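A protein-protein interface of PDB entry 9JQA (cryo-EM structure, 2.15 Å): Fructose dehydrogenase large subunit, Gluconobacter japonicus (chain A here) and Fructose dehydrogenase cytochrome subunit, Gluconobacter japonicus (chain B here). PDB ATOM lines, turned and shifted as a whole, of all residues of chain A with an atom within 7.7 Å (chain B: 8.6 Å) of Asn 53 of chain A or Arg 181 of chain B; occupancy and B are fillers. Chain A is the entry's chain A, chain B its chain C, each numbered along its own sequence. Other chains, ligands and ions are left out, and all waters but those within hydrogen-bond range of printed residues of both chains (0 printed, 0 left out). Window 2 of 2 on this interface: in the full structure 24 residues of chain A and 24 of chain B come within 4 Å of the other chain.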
ATOM      1  N   GLN A  46       6.867 -15.894 -11.436  1.00  0.00           N
ATOM      2  CA  GLN A  46       7.508 -16.093 -12.731  1.00  0.00           C
ATOM      3  C   GLN A  46       8.666 -15.125 -12.925  1.00  0.00           C
ATOM      4  O   GLN A  46       9.709 -15.501 -13.463  1.00  0.00           O
ATOM      5  CB  GLN A  46       6.492 -15.949 -13.859  1.00  0.00           C
ATOM      6  CG  GLN A  46       7.045 -16.341 -15.215  1.00  0.00           C
ATOM      7  CD  GLN A  46       7.644 -17.730 -15.218  1.00  0.00           C
ATOM      8  OE1 GLN A  46       7.008 -18.692 -14.797  1.00  0.00           O
ATOM      9  NE2 GLN A  46       8.875 -17.841 -15.694  1.00  0.00           N
ATOM     10  N   ILE A  47       8.501 -13.873 -12.494  1.00  0.00           N
ATOM     11  CA  ILE A  47       9.599 -12.916 -12.574  1.00  0.00           C
ATOM     12  C   ILE A  47      10.749 -13.355 -11.678  1.00  0.00           C
ATOM     13  O   ILE A  47      11.923 -13.184 -12.021  1.00  0.00           O
ATOM     14  CB  ILE A  47       9.110 -11.501 -12.212  1.00  0.00           C
ATOM     15  CG1 ILE A  47       7.895 -11.119 -13.057  1.00  0.00           C
ATOM     16  CG2 ILE A  47      10.222 -10.498 -12.408  1.00  0.00           C
ATOM     17  CD1 ILE A  47       8.115 -11.240 -14.545  1.00  0.00           C
ATOM     18  N   VAL A  48      10.429 -13.928 -10.518  1.00  0.00           N
ATOM     19  CA  VAL A  48      11.465 -14.441  -9.627  1.00  0.00           C
ATOM     20  C   VAL A  48      12.234 -15.569 -10.299  1.00  0.00           C
ATOM     21  O   VAL A  48      13.468 -15.618 -10.245  1.00  0.00           O
ATOM     22  CB  VAL A  48      10.839 -14.898  -8.298  1.00  0.00           C
ATOM     23  CG1 VAL A  48      11.859 -15.632  -7.455  1.00  0.00           C
ATOM     24  CG2 VAL A  48      10.292 -13.712  -7.556  1.00  0.00           C
ATOM     25  N   GLU A  49      11.517 -16.493 -10.939  1.00  0.00           N
ATOM     26  CA  GLU A  49      12.183 -17.580 -11.649  1.00  0.00           C
ATOM     27  C   GLU A  49      13.037 -17.051 -12.792  1.00  0.00           C
ATOM     28  O   GLU A  49      14.145 -17.543 -13.028  1.00  0.00           O
ATOM     29  CB  GLU A  49      11.153 -18.580 -12.172  1.00  0.00           C
ATOM     30  CG  GLU A  49      11.760 -19.894 -12.618  1.00  0.00           C
ATOM     31  CD  GLU A  49      10.837 -20.693 -13.510  1.00  0.00           C
ATOM     32  OE1 GLU A  49      10.663 -20.310 -14.684  1.00  0.00           O
ATOM     33  OE2 GLU A  49      10.286 -21.707 -13.039  1.00  0.00           O
ATOM     34  N   ASN A  50      12.534 -16.050 -13.518  1.00  0.00           N
ATOM     35  CA  ASN A  50      13.300 -15.466 -14.611  1.00  0.00           C
ATOM     36  C   ASN A  50      14.576 -14.812 -14.101  1.00  0.00           C
ATOM     37  O   ASN A  50      15.635 -14.933 -14.723  1.00  0.00           O
ATOM     38  CB  ASN A  50      12.448 -14.453 -15.371  1.00  0.00           C
ATOM     39  CG  ASN A  50      11.297 -15.095 -16.107  1.00  0.00           C
ATOM     40  OD1 ASN A  50      11.214 -16.315 -16.210  1.00  0.00           O
ATOM     41  ND2 ASN A  50      10.396 -14.272 -16.622  1.00  0.00           N
ATOM     42  N   TRP A  51      14.492 -14.102 -12.975  1.00  0.00           N
ATOM     43  CA  TRP A  51      15.684 -13.481 -12.413  1.00  0.00           C
ATOM     44  C   TRP A  51      16.671 -14.528 -11.918  1.00  0.00           C
ATOM     45  O   TRP A  51      17.884 -14.364 -12.077  1.00  0.00           O
ATOM     46  CB  TRP A  51      15.320 -12.527 -11.279  1.00  0.00           C
ATOM     47  CG  TRP A  51      16.529 -11.852 -10.724  1.00  0.00           C
ATOM     48  CD1 TRP A  51      17.085 -10.690 -11.157  1.00  0.00           C
ATOM     49  CD2 TRP A  51      17.357 -12.317  -9.654  1.00  0.00           C
ATOM     50  NE1 TRP A  51      18.199 -10.391 -10.416  1.00  0.00           N
ATOM     51  CE2 TRP A  51      18.390 -11.378  -9.487  1.00  0.00           C
ATOM     52  CE3 TRP A  51      17.323 -13.434  -8.817  1.00  0.00           C
ATOM     53  CZ2 TRP A  51      19.374 -11.519  -8.519  1.00  0.00           C
ATOM     54  CZ3 TRP A  51      18.301 -13.573  -7.861  1.00  0.00           C
ATOM     55  CH2 TRP A  51      19.313 -12.622  -7.718  1.00  0.00           C
ATOM     56  N   ARG A  52      16.172 -15.604 -11.307  1.00  0.00           N
ATOM     57  CA  ARG A  52      17.059 -16.656 -10.825  1.00  0.00           C
ATOM     58  C   ARG A  52      17.808 -17.310 -11.975  1.00  0.00           C
ATOM     59  O   ARG A  52      18.982 -17.667 -11.838  1.00  0.00           O
ATOM     60  CB  ARG A  52      16.263 -17.698 -10.043  1.00  0.00           C
ATOM     61  CG  ARG A  52      15.875 -17.257  -8.650  1.00  0.00           C
ATOM     62  CD  ARG A  52      14.866 -18.201  -8.041  1.00  0.00           C
ATOM     63  NE  ARG A  52      14.558 -17.853  -6.661  1.00  0.00           N
ATOM     64  CZ  ARG A  52      13.511 -18.310  -5.992  1.00  0.00           C
ATOM     65  NH1 ARG A  52      12.653 -19.151  -6.544  1.00  0.00           N
ATOM     66  NH2 ARG A  52      13.317 -17.913  -4.740  1.00  0.00           N
ATOM     67  N   ASN A  53      17.147 -17.476 -13.115  1.00  0.00           N
ATOM     68  CA  ASN A  53      17.757 -18.065 -14.295  1.00  0.00           C
ATOM     69  C   ASN A  53      18.393 -17.028 -15.207  1.00  0.00           C
ATOM     70  O   ASN A  53      18.830 -17.373 -16.308  1.00  0.00           O
ATOM     71  CB  ASN A  53      16.722 -18.883 -15.065  1.00  0.00           C
ATOM     72  CG  ASN A  53      16.673 -20.323 -14.609  1.00  0.00           C
ATOM     73  OD1 ASN A  53      16.100 -20.635 -13.569  1.00  0.00           O
ATOM     74  ND2 ASN A  53      17.280 -21.209 -15.384  1.00  0.00           N
ATOM     75  N   MET A  54      18.431 -15.770 -14.789  1.00  0.00           N
ATOM     76  CA  MET A  54      19.215 -14.773 -15.498  1.00  0.00           C
ATOM     77  C   MET A  54      20.702 -15.035 -15.268  1.00  0.00           C
ATOM     78  O   MET A  54      21.096 -15.441 -14.171  1.00  0.00           O
ATOM     79  CB  MET A  54      18.830 -13.373 -15.024  1.00  0.00           C
ATOM     80  CG  MET A  54      19.060 -12.265 -16.033  1.00  0.00           C
ATOM     81  SD  MET A  54      18.753 -10.640 -15.327  1.00  0.00           S
ATOM     82  CE  MET A  54      19.786 -10.718 -13.876  1.00  0.00           C
ATOM     83  N   PRO A  55      21.545 -14.835 -16.280  1.00  0.00           N
ATOM     84  CA  PRO A  55      22.960 -15.152 -16.122  1.00  0.00           C
ATOM     85  C   PRO A  55      23.584 -14.323 -15.019  1.00  0.00           C
ATOM     86  O   PRO A  55      23.174 -13.174 -14.770  1.00  0.00           O
ATOM     87  CB  PRO A  55      23.552 -14.805 -17.493  1.00  0.00           C
ATOM     88  CG  PRO A  55      22.426 -14.979 -18.422  1.00  0.00           C
ATOM     89  CD  PRO A  55      21.210 -14.524 -17.678  1.00  0.00           C
ATOM     90  N   PRO A  56      24.580 -14.871 -14.319  1.00  0.00           N
ATOM     91  CA  PRO A  56      25.179 -14.141 -13.193  1.00  0.00           C
ATOM     92  C   PRO A  56      25.836 -12.833 -13.586  1.00  0.00           C
ATOM     93  O   PRO A  56      25.963 -11.945 -12.739  1.00  0.00           O
ATOM     94  CB  PRO A  56      26.201 -15.142 -12.640  1.00  0.00           C
ATOM     95  CG  PRO A  56      26.505 -16.036 -13.778  1.00  0.00           C
ATOM     96  CD  PRO A  56      25.226 -16.174 -14.533  1.00  0.00           C
ATOM     97  N   LYS A  59      23.318 -10.352 -13.142  1.00  0.00           N
ATOM     98  CA  LYS A  59      23.066 -10.038 -11.742  1.00  0.00           C
ATOM     99  C   LYS A  59      24.148  -9.133 -11.173  1.00  0.00           C
ATOM    100  O   LYS A  59      23.845  -8.201 -10.422  1.00  0.00           O
ATOM    101  CB  LYS A  59      22.980 -11.319 -10.910  1.00  0.00           C
ATOM    102  CG  LYS A  59      21.836 -12.245 -11.264  1.00  0.00           C
ATOM    103  CD  LYS A  59      21.873 -13.486 -10.392  1.00  0.00           C
ATOM    104  CE  LYS A  59      20.655 -14.358 -10.599  1.00  0.00           C
ATOM    105  NZ  LYS A  59      20.982 -15.596 -11.350  1.00  0.00           N
ATOM    106  N   THR A  66      15.600  -7.668 -17.745  1.00  0.00           N
ATOM    107  CA  THR A  66      15.538  -9.008 -18.324  1.00  0.00           C
ATOM    108  C   THR A  66      14.524  -9.925 -17.647  1.00  0.00           C
ATOM    109  O   THR A  66      13.833 -10.664 -18.370  1.00  0.00           O
ATOM    110  CB  THR A  66      16.937  -9.636 -18.313  1.00  0.00           C
ATOM    111  OG1 THR A  66      17.809  -8.862 -19.144  1.00  0.00           O
ATOM    112  CG2 THR A  66      16.897 -11.059 -18.834  1.00  0.00           C
ATOM    113  N   PRO A  67      14.372  -9.944 -16.317  1.00  0.00           N
ATOM    114  CA  PRO A  67      13.335 -10.804 -15.726  1.00  0.00           C
ATOM    115  C   PRO A  67      11.932 -10.486 -16.202  1.00  0.00           C
ATOM    116  O   PRO A  67      11.053 -11.351 -16.104  1.00  0.00           O
ATOM    117  CB  PRO A  67      13.488 -10.553 -14.222  1.00  0.00           C
ATOM    118  CG  PRO A  67      14.887 -10.143 -14.063  1.00  0.00           C
ATOM    119  CD  PRO A  67      15.204  -9.328 -15.269  1.00  0.00           C
ATOM    120  N   PRO A  69       9.833  -9.996 -19.395  1.00  0.00           N
ATOM    121  CA  PRO A  69       9.896 -10.090 -20.858  1.00  0.00           C
ATOM    122  C   PRO A  69       9.213  -8.902 -21.515  1.00  0.00           C
ATOM    123  O   PRO A  69       8.080  -8.550 -21.184  1.00  0.00           O
ATOM    124  CB  PRO A  69       9.165 -11.403 -21.159  1.00  0.00           C
ATOM    125  CG  PRO A  69       9.182 -12.154 -19.873  1.00  0.00           C
ATOM    126  CD  PRO A  69       9.114 -11.131 -18.801  1.00  0.00           C
ATOM    127  N   TYR B 172      13.856 -30.249  -8.132  1.00  0.00           N
ATOM    128  CA  TYR B 172      13.834 -29.043  -8.945  1.00  0.00           C
ATOM    129  C   TYR B 172      15.056 -28.986  -9.851  1.00  0.00           C
ATOM    130  O   TYR B 172      16.162 -29.356  -9.450  1.00  0.00           O
ATOM    131  CB  TYR B 172      13.782 -27.799  -8.061  1.00  0.00           C
ATOM    132  CG  TYR B 172      13.863 -26.503  -8.830  1.00  0.00           C
ATOM    133  CD1 TYR B 172      12.861 -26.136  -9.713  1.00  0.00           C
ATOM    134  CD2 TYR B 172      14.943 -25.648  -8.674  1.00  0.00           C
ATOM    135  CE1 TYR B 172      12.930 -24.955 -10.418  1.00  0.00           C
ATOM    136  CE2 TYR B 172      15.021 -24.465  -9.374  1.00  0.00           C
ATOM    137  CZ  TYR B 172      14.011 -24.123 -10.244  1.00  0.00           C
ATOM    138  OH  TYR B 172      14.083 -22.944 -10.945  1.00  0.00           O
ATOM    139  N   SER B 173      14.848 -28.517 -11.076  1.00  0.00           N
ATOM    140  CA  SER B 173      15.915 -28.357 -12.054  1.00  0.00           C
ATOM    141  C   SER B 173      16.008 -26.888 -12.436  1.00  0.00           C
ATOM    142  O   SER B 173      15.043 -26.318 -12.954  1.00  0.00           O
ATOM    143  CB  SER B 173      15.661 -29.221 -13.289  1.00  0.00           C
ATOM    144  OG  SER B 173      16.745 -29.146 -14.195  1.00  0.00           O
ATOM    145  N   VAL B 174      17.164 -26.279 -12.173  1.00  0.00           N
ATOM    146  CA  VAL B 174      17.386 -24.904 -12.603  1.00  0.00           C
ATOM    147  C   VAL B 174      17.491 -24.837 -14.120  1.00  0.00           C
ATOM    148  O   VAL B 174      16.976 -23.907 -14.751  1.00  0.00           O
ATOM    149  CB  VAL B 174      18.639 -24.329 -11.919  1.00  0.00           C
ATOM    150  CG1 VAL B 174      19.060 -23.028 -12.571  1.00  0.00           C
ATOM    151  CG2 VAL B 174      18.381 -24.122 -10.445  1.00  0.00           C
ATOM    152  N   ALA B 175      18.143 -25.828 -14.729  1.00  0.00           N
ATOM    153  CA  ALA B 175      18.317 -25.826 -16.177  1.00  0.00           C
ATOM    154  C   ALA B 175      16.978 -25.875 -16.899  1.00  0.00           C
ATOM    155  O   ALA B 175      16.763 -25.144 -17.872  1.00  0.00           O
ATOM    156  CB  ALA B 175      19.197 -27.001 -16.597  1.00  0.00           C
ATOM    157  N   ASN B 176      16.058 -26.717 -16.423  1.00  0.00           N
ATOM    158  CA  ASN B 176      14.767 -26.859 -17.085  1.00  0.00           C
ATOM    159  C   ASN B 176      13.943 -25.582 -17.035  1.00  0.00           C
ATOM    160  O   ASN B 176      13.029 -25.417 -17.849  1.00  0.00           O
ATOM    161  CB  ASN B 176      13.987 -28.014 -16.460  1.00  0.00           C
ATOM    162  CG  ASN B 176      14.464 -29.363 -16.946  1.00  0.00           C
ATOM    163  OD1 ASN B 176      15.170 -29.459 -17.948  1.00  0.00           O
ATOM    164  ND2 ASN B 176      14.082 -30.416 -16.237  1.00  0.00           N
ATOM    165  N   ALA B 177      14.241 -24.679 -16.106  1.00  0.00           N
ATOM    166  CA  ALA B 177      13.557 -23.396 -16.051  1.00  0.00           C
ATOM    167  C   ALA B 177      14.004 -22.439 -17.146  1.00  0.00           C
ATOM    168  O   ALA B 177      13.315 -21.444 -17.391  1.00  0.00           O
ATOM    169  CB  ALA B 177      13.768 -22.744 -14.685  1.00  0.00           C
ATOM    170  N   ASN B 178      15.128 -22.718 -17.811  1.00  0.00           N
ATOM    171  CA  ASN B 178      15.639 -21.797 -18.821  1.00  0.00           C
ATOM    172  C   ASN B 178      14.674 -21.644 -19.986  1.00  0.00           C
ATOM    173  O   ASN B 178      14.596 -20.569 -20.588  1.00  0.00           O
ATOM    174  CB  ASN B 178      16.999 -22.271 -19.323  1.00  0.00           C
ATOM    175  CG  ASN B 178      18.103 -22.022 -18.325  1.00  0.00           C
ATOM    176  OD1 ASN B 178      18.297 -20.900 -17.866  1.00  0.00           O
ATOM    177  ND2 ASN B 178      18.831 -23.072 -17.977  1.00  0.00           N
ATOM    178  N   SER B 179      13.938 -22.704 -20.324  1.00  0.00           N
ATOM    179  CA  SER B 179      12.951 -22.604 -21.389  1.00  0.00           C
ATOM    180  C   SER B 179      11.772 -21.724 -21.001  1.00  0.00           C
ATOM    181  O   SER B 179      11.070 -21.226 -21.884  1.00  0.00           O
ATOM    182  CB  SER B 179      12.452 -23.994 -21.778  1.00  0.00           C
ATOM    183  OG  SER B 179      11.651 -24.551 -20.754  1.00  0.00           O
ATOM    184  N   ARG B 180      11.542 -21.520 -19.707  1.00  0.00           N
ATOM    185  CA  ARG B 180      10.423 -20.710 -19.249  1.00  0.00           C
ATOM    186  C   ARG B 180      10.783 -19.242 -19.089  1.00  0.00           C
ATOM    187  O   ARG B 180       9.926 -18.452 -18.685  1.00  0.00           O
ATOM    188  CB  ARG B 180       9.876 -21.259 -17.931  1.00  0.00           C
ATOM    189  CG  ARG B 180       9.143 -22.572 -18.087  1.00  0.00           C
ATOM    190  CD  ARG B 180       8.410 -22.937 -16.821  1.00  0.00           C
ATOM    191  NE  ARG B 180       9.323 -23.123 -15.703  1.00  0.00           N
ATOM    192  CZ  ARG B 180       9.982 -24.245 -15.456  1.00  0.00           C
ATOM    193  NH1 ARG B 180       9.855 -25.306 -16.233  1.00  0.00           N
ATOM    194  NH2 ARG B 180      10.793 -24.303 -14.405  1.00  0.00           N
ATOM    195  N   ARG B 181      12.018 -18.858 -19.384  1.00  0.00           N
ATOM    196  CA  ARG B 181      12.323 -17.444 -19.500  1.00  0.00           C
ATOM    197  C   ARG B 181      11.597 -16.879 -20.715  1.00  0.00           C
ATOM    198  O   ARG B 181      11.143 -17.615 -21.595  1.00  0.00           O
ATOM    199  CB  ARG B 181      13.830 -17.219 -19.610  1.00  0.00           C
ATOM    200  CG  ARG B 181      14.607 -17.714 -18.405  1.00  0.00           C
ATOM    201  CD  ARG B 181      16.099 -17.527 -18.581  1.00  0.00           C
ATOM    202  NE  ARG B 181      16.596 -18.193 -19.777  1.00  0.00           N
ATOM    203  CZ  ARG B 181      17.874 -18.259 -20.121  1.00  0.00           C
ATOM    204  NH1 ARG B 181      18.820 -17.717 -19.372  1.00  0.00           N
ATOM    205  NH2 ARG B 181      18.212 -18.885 -21.244  1.00  0.00           N
ATOM    206  N   SER B 182      11.473 -15.556 -20.745  1.00  0.00           N
ATOM    207  CA  SER B 182      10.624 -14.853 -21.706  1.00  0.00           C
ATOM    208  C   SER B 182       9.150 -15.192 -21.519  1.00  0.00           C
ATOM    209  O   SER B 182       8.337 -14.962 -22.417  1.00  0.00           O
ATOM    210  CB  SER B 182      11.049 -15.125 -23.154  1.00  0.00           C
ATOM    211  OG  SER B 182      10.452 -16.311 -23.640  1.00  0.00           O
ATOM    212  N   ASN B 183       8.791 -15.732 -20.359  1.00  0.00           N
ATOM    213  CA  ASN B 183       7.405 -15.896 -19.946  1.00  0.00           C
ATOM    214  C   ASN B 183       7.114 -14.899 -18.835  1.00  0.00           C
ATOM    215  O   ASN B 183       7.931 -14.726 -17.927  1.00  0.00           O
ATOM    216  CB  ASN B 183       7.129 -17.317 -19.453  1.00  0.00           C
ATOM    217  CG  ASN B 183       6.954 -18.303 -20.581  1.00  0.00           C
ATOM    218  OD1 ASN B 183       6.888 -17.925 -21.749  1.00  0.00           O
ATOM    219  ND2 ASN B 183       6.873 -19.580 -20.238  1.00  0.00           N
ATOM    220  N   SER B 184       5.965 -14.239 -18.915  1.00  0.00           N
ATOM    221  CA  SER B 184       5.594 -13.252 -17.913  1.00  0.00           C
ATOM    222  C   SER B 184       4.691 -13.811 -16.823  1.00  0.00           C
ATOM    223  O   SER B 184       4.516 -13.154 -15.793  1.00  0.00           O
ATOM    224  CB  SER B 184       4.909 -12.055 -18.578  1.00  0.00           C
ATOM    225  OG  SER B 184       5.555 -11.701 -19.786  1.00  0.00           O
ATOM    226  N   THR B 185       4.123 -14.998 -17.014  1.00  0.00           N
ATOM    227  CA  THR B 185       3.212 -15.583 -16.043  1.00  0.00           C
ATOM    228  C   THR B 185       3.581 -17.040 -15.810  1.00  0.00           C
ATOM    229  O   THR B 185       4.342 -17.642 -16.570  1.00  0.00           O
ATOM    230  CB  THR B 185       1.750 -15.487 -16.494  1.00  0.00           C
ATOM    231  OG1 THR B 185       1.624 -15.995 -17.827  1.00  0.00           O
ATOM    232  CG2 THR B 185       1.276 -14.048 -16.460  1.00  0.00           C
ATOM    233  N   LYS B 188       2.601 -21.524 -17.982  1.00  0.00           N
ATOM    234  CA  LYS B 188       3.331 -22.621 -18.596  1.00  0.00           C
ATOM    235  C   LYS B 188       4.274 -23.318 -17.623  1.00  0.00           C
ATOM    236  O   LYS B 188       5.011 -24.218 -18.034  1.00  0.00           O
ATOM    237  CB  LYS B 188       4.109 -22.117 -19.813  1.00  0.00           C
ATOM    238  CG  LYS B 188       3.211 -21.610 -20.928  1.00  0.00           C
ATOM    239  CD  LYS B 188       3.941 -21.533 -22.252  1.00  0.00           C
ATOM    240  CE  LYS B 188       3.641 -20.228 -22.967  1.00  0.00           C
ATOM    241  NZ  LYS B 188       4.736 -19.834 -23.892  1.00  0.00           N
ATOM    242  N   THR B 189       4.265 -22.922 -16.353  1.00  0.00           N
ATOM    243  CA  THR B 189       5.028 -23.591 -15.301  1.00  0.00           C
ATOM    244  C   THR B 189       4.082 -24.567 -14.612  1.00  0.00           C
ATOM    245  O   THR B 189       3.393 -24.220 -13.654  1.00  0.00           O
ATOM    246  CB  THR B 189       5.604 -22.584 -14.315  1.00  0.00           C
ATOM    247  OG1 THR B 189       6.235 -21.514 -15.030  1.00  0.00           O
ATOM    248  CG2 THR B 189       6.620 -23.249 -13.407  1.00  0.00           C
ATOM    249  N   GLU B 197       9.465 -23.946  -6.144  1.00  0.00           N
ATOM    250  CA  GLU B 197      10.665 -23.121  -6.099  1.00  0.00           C
ATOM    251  C   GLU B 197      10.348 -21.658  -6.379  1.00  0.00           C
ATOM    252  O   GLU B 197      10.881 -20.765  -5.714  1.00  0.00           O
ATOM    253  CB  GLU B 197      11.704 -23.643  -7.087  1.00  0.00           C
ATOM    254  CG  GLU B 197      13.072 -23.027  -6.906  1.00  0.00           C
ATOM    255  CD  GLU B 197      13.895 -23.736  -5.854  1.00  0.00           C
ATOM    256  OE1 GLU B 197      13.476 -24.819  -5.400  1.00  0.00           O
ATOM    257  OE2 GLU B 197      14.963 -23.214  -5.482  1.00  0.00           O
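NE2 of Gln 46 of chain A is in hydrogen-bond range of O of Arg 180 of chain B.
The backbone carbonyl oxygen (O) of Thr 185 of chain B lies close to the side-chain amide oxygen (OE1) of Gln 46 of chain A.
The side-chain hydroxyl of Thr 189 of chain B is in hydrogen-bond range of the side-chain amide oxygen of Gln 46 of chain A, 2.9 Å away.
OE2 of Glu 49 of chain A is in salt-bridge range of NH2 of Arg 180 of chain B (3.0 Å).
The side-chain amide nitrogen of Asn 50 of chain A lies within hydrogen-bond range of the backbone carbonyl oxygen of Asn 183 of chain B, at 2.8 Å.
The backbone carbonyl oxygen (O) of Glu 197 of chain B sits at hydrogen-bond distance from the guanidinium group (NH1) of Arg 52 of chain A (2.5 Å).
The side-chain amide nitrogen (ND2) of Asn 53 of chain A sits at hydrogen-bond distance from the backbone carbonyl oxygen (O) of Val 174 of chain B.
The side-chain amide nitrogen (ND2) of Asn 53 of chain A is in hydrogen-bond range of the side-chain amide oxygen (OD1) of Asn 178 of chain B.
The guanidinium group (NH1) of Arg 181 of chain B is in hydrogen-bond range of the backbone carbonyl oxygen (O) of Asn 53 of chain A, at 3.1 Å.
NE2 of Gln 46 of chain A lies within hydrogen-bond range of OE1 of Glu 49 of chain A, at 3.2 Å.
The side-chain amide nitrogen of Gln 46 of chain A is in hydrogen-bond range of the side-chain amide oxygen of Asn 50 of chain A (2.8 Å).
The backbone carbonyl oxygen of Pro 67 of chain A sits at hydrogen-bond distance from the side-chain amide nitrogen of Asn 50 of chain A, 3.0 Å away.
O of Arg 52 of chain A is in hydrogen-bond range of NZ of Lys 59 of chain A (2.9 Å).
O of Ala 175 of chain B lies within hydrogen-bond range of ND2 of Asn 178 of chain B (2.9 Å).
O of Asn 178 of chain B is in hydrogen-bond range of NE of Arg 181 of chain B, 3.2 Å away.
Among the printed residues, merely in contact across the chains: Gln 46 of chain A with Asn 183 of chain B (3.3 Å), Gln 46 of chain A with Ser 184 of chain B (3.8 Å), Glu 49 of chain A with Ala 177 of chain B (3.8 Å), Glu 49 of chain A with Thr 189 of chain B (3.99 Å), Asn 50 of chain A with Arg 180 of chain B (3.5 Å), Asn 50 of chain A with Arg 181 of chain B (3.7 Å), Asn 53 of chain A with Ala 177 of chain B (3.3 Å), Pro 69 of chain A with Ser 182 of chain B (3.5 Å), Pro 69 of chain A with Asn 183 of chain B (3.5 Å) and Pro 69 of chain A with Ser 184 of chain B (3.7 Å).
Of the printed residues of chain B, Gln 46 of chain A touches Arg 180 (3.2 Å), Asn 183 (3.3 Å), Ser 184 (3.8 Å), Thr 185 (3.3 Å) and Thr 189 (2.9 Å).
Of the printed residues of chain B, Glu 49 of chain A touches Ala 177 (3.8 Å), Arg 180 (3.0 Å) and Thr 189 (3.99 Å).
Asn 53 of chain A touches just these residues of chain B: Val 174 (2.8 Å), Ala 177 (3.3 Å), Asn 178 (2.7 Å) and Arg 181 (3.1 Å).
Tyr 172 of chain B touches none of the printed residues of chain A.
Of the printed residues of chain A, Ala 177 of chain B touches Glu 49 (3.8 Å) and Asn 53 (3.3 Å).
Of the printed residues of chain A, Asn 178 of chain B touches Asn 53 (2.7 Å).
Of chain A, only Asn 50 and Asn 53 come within 4 Å of Arg 181 of chain B.
Printed residues of chain A within 4 Å of Ser 184 of chain B: Gln 46 (3.8 Å) and Pro 69 (3.7 Å).
The nearest residue of chain A that does not touch Arg 181 of chain B is Pro 55 of chain A (4.3 Å).
Of the 17 printed residues of chain B, 11 touch a printed residue of chain A.
Of the 15 printed residues of chain A, 6 touch a printed residue of chain B.
Hydrophobic or aromatic side chains of chain A that line the printed part of chain B: Pro 69.
Among the printed residues, Asp or Glu carboxylates within 4 Å of a Lys or Arg side-chain nitrogen of the other chain: Glu 49 of chain A with Arg 180 of chain B (3.0 Å).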
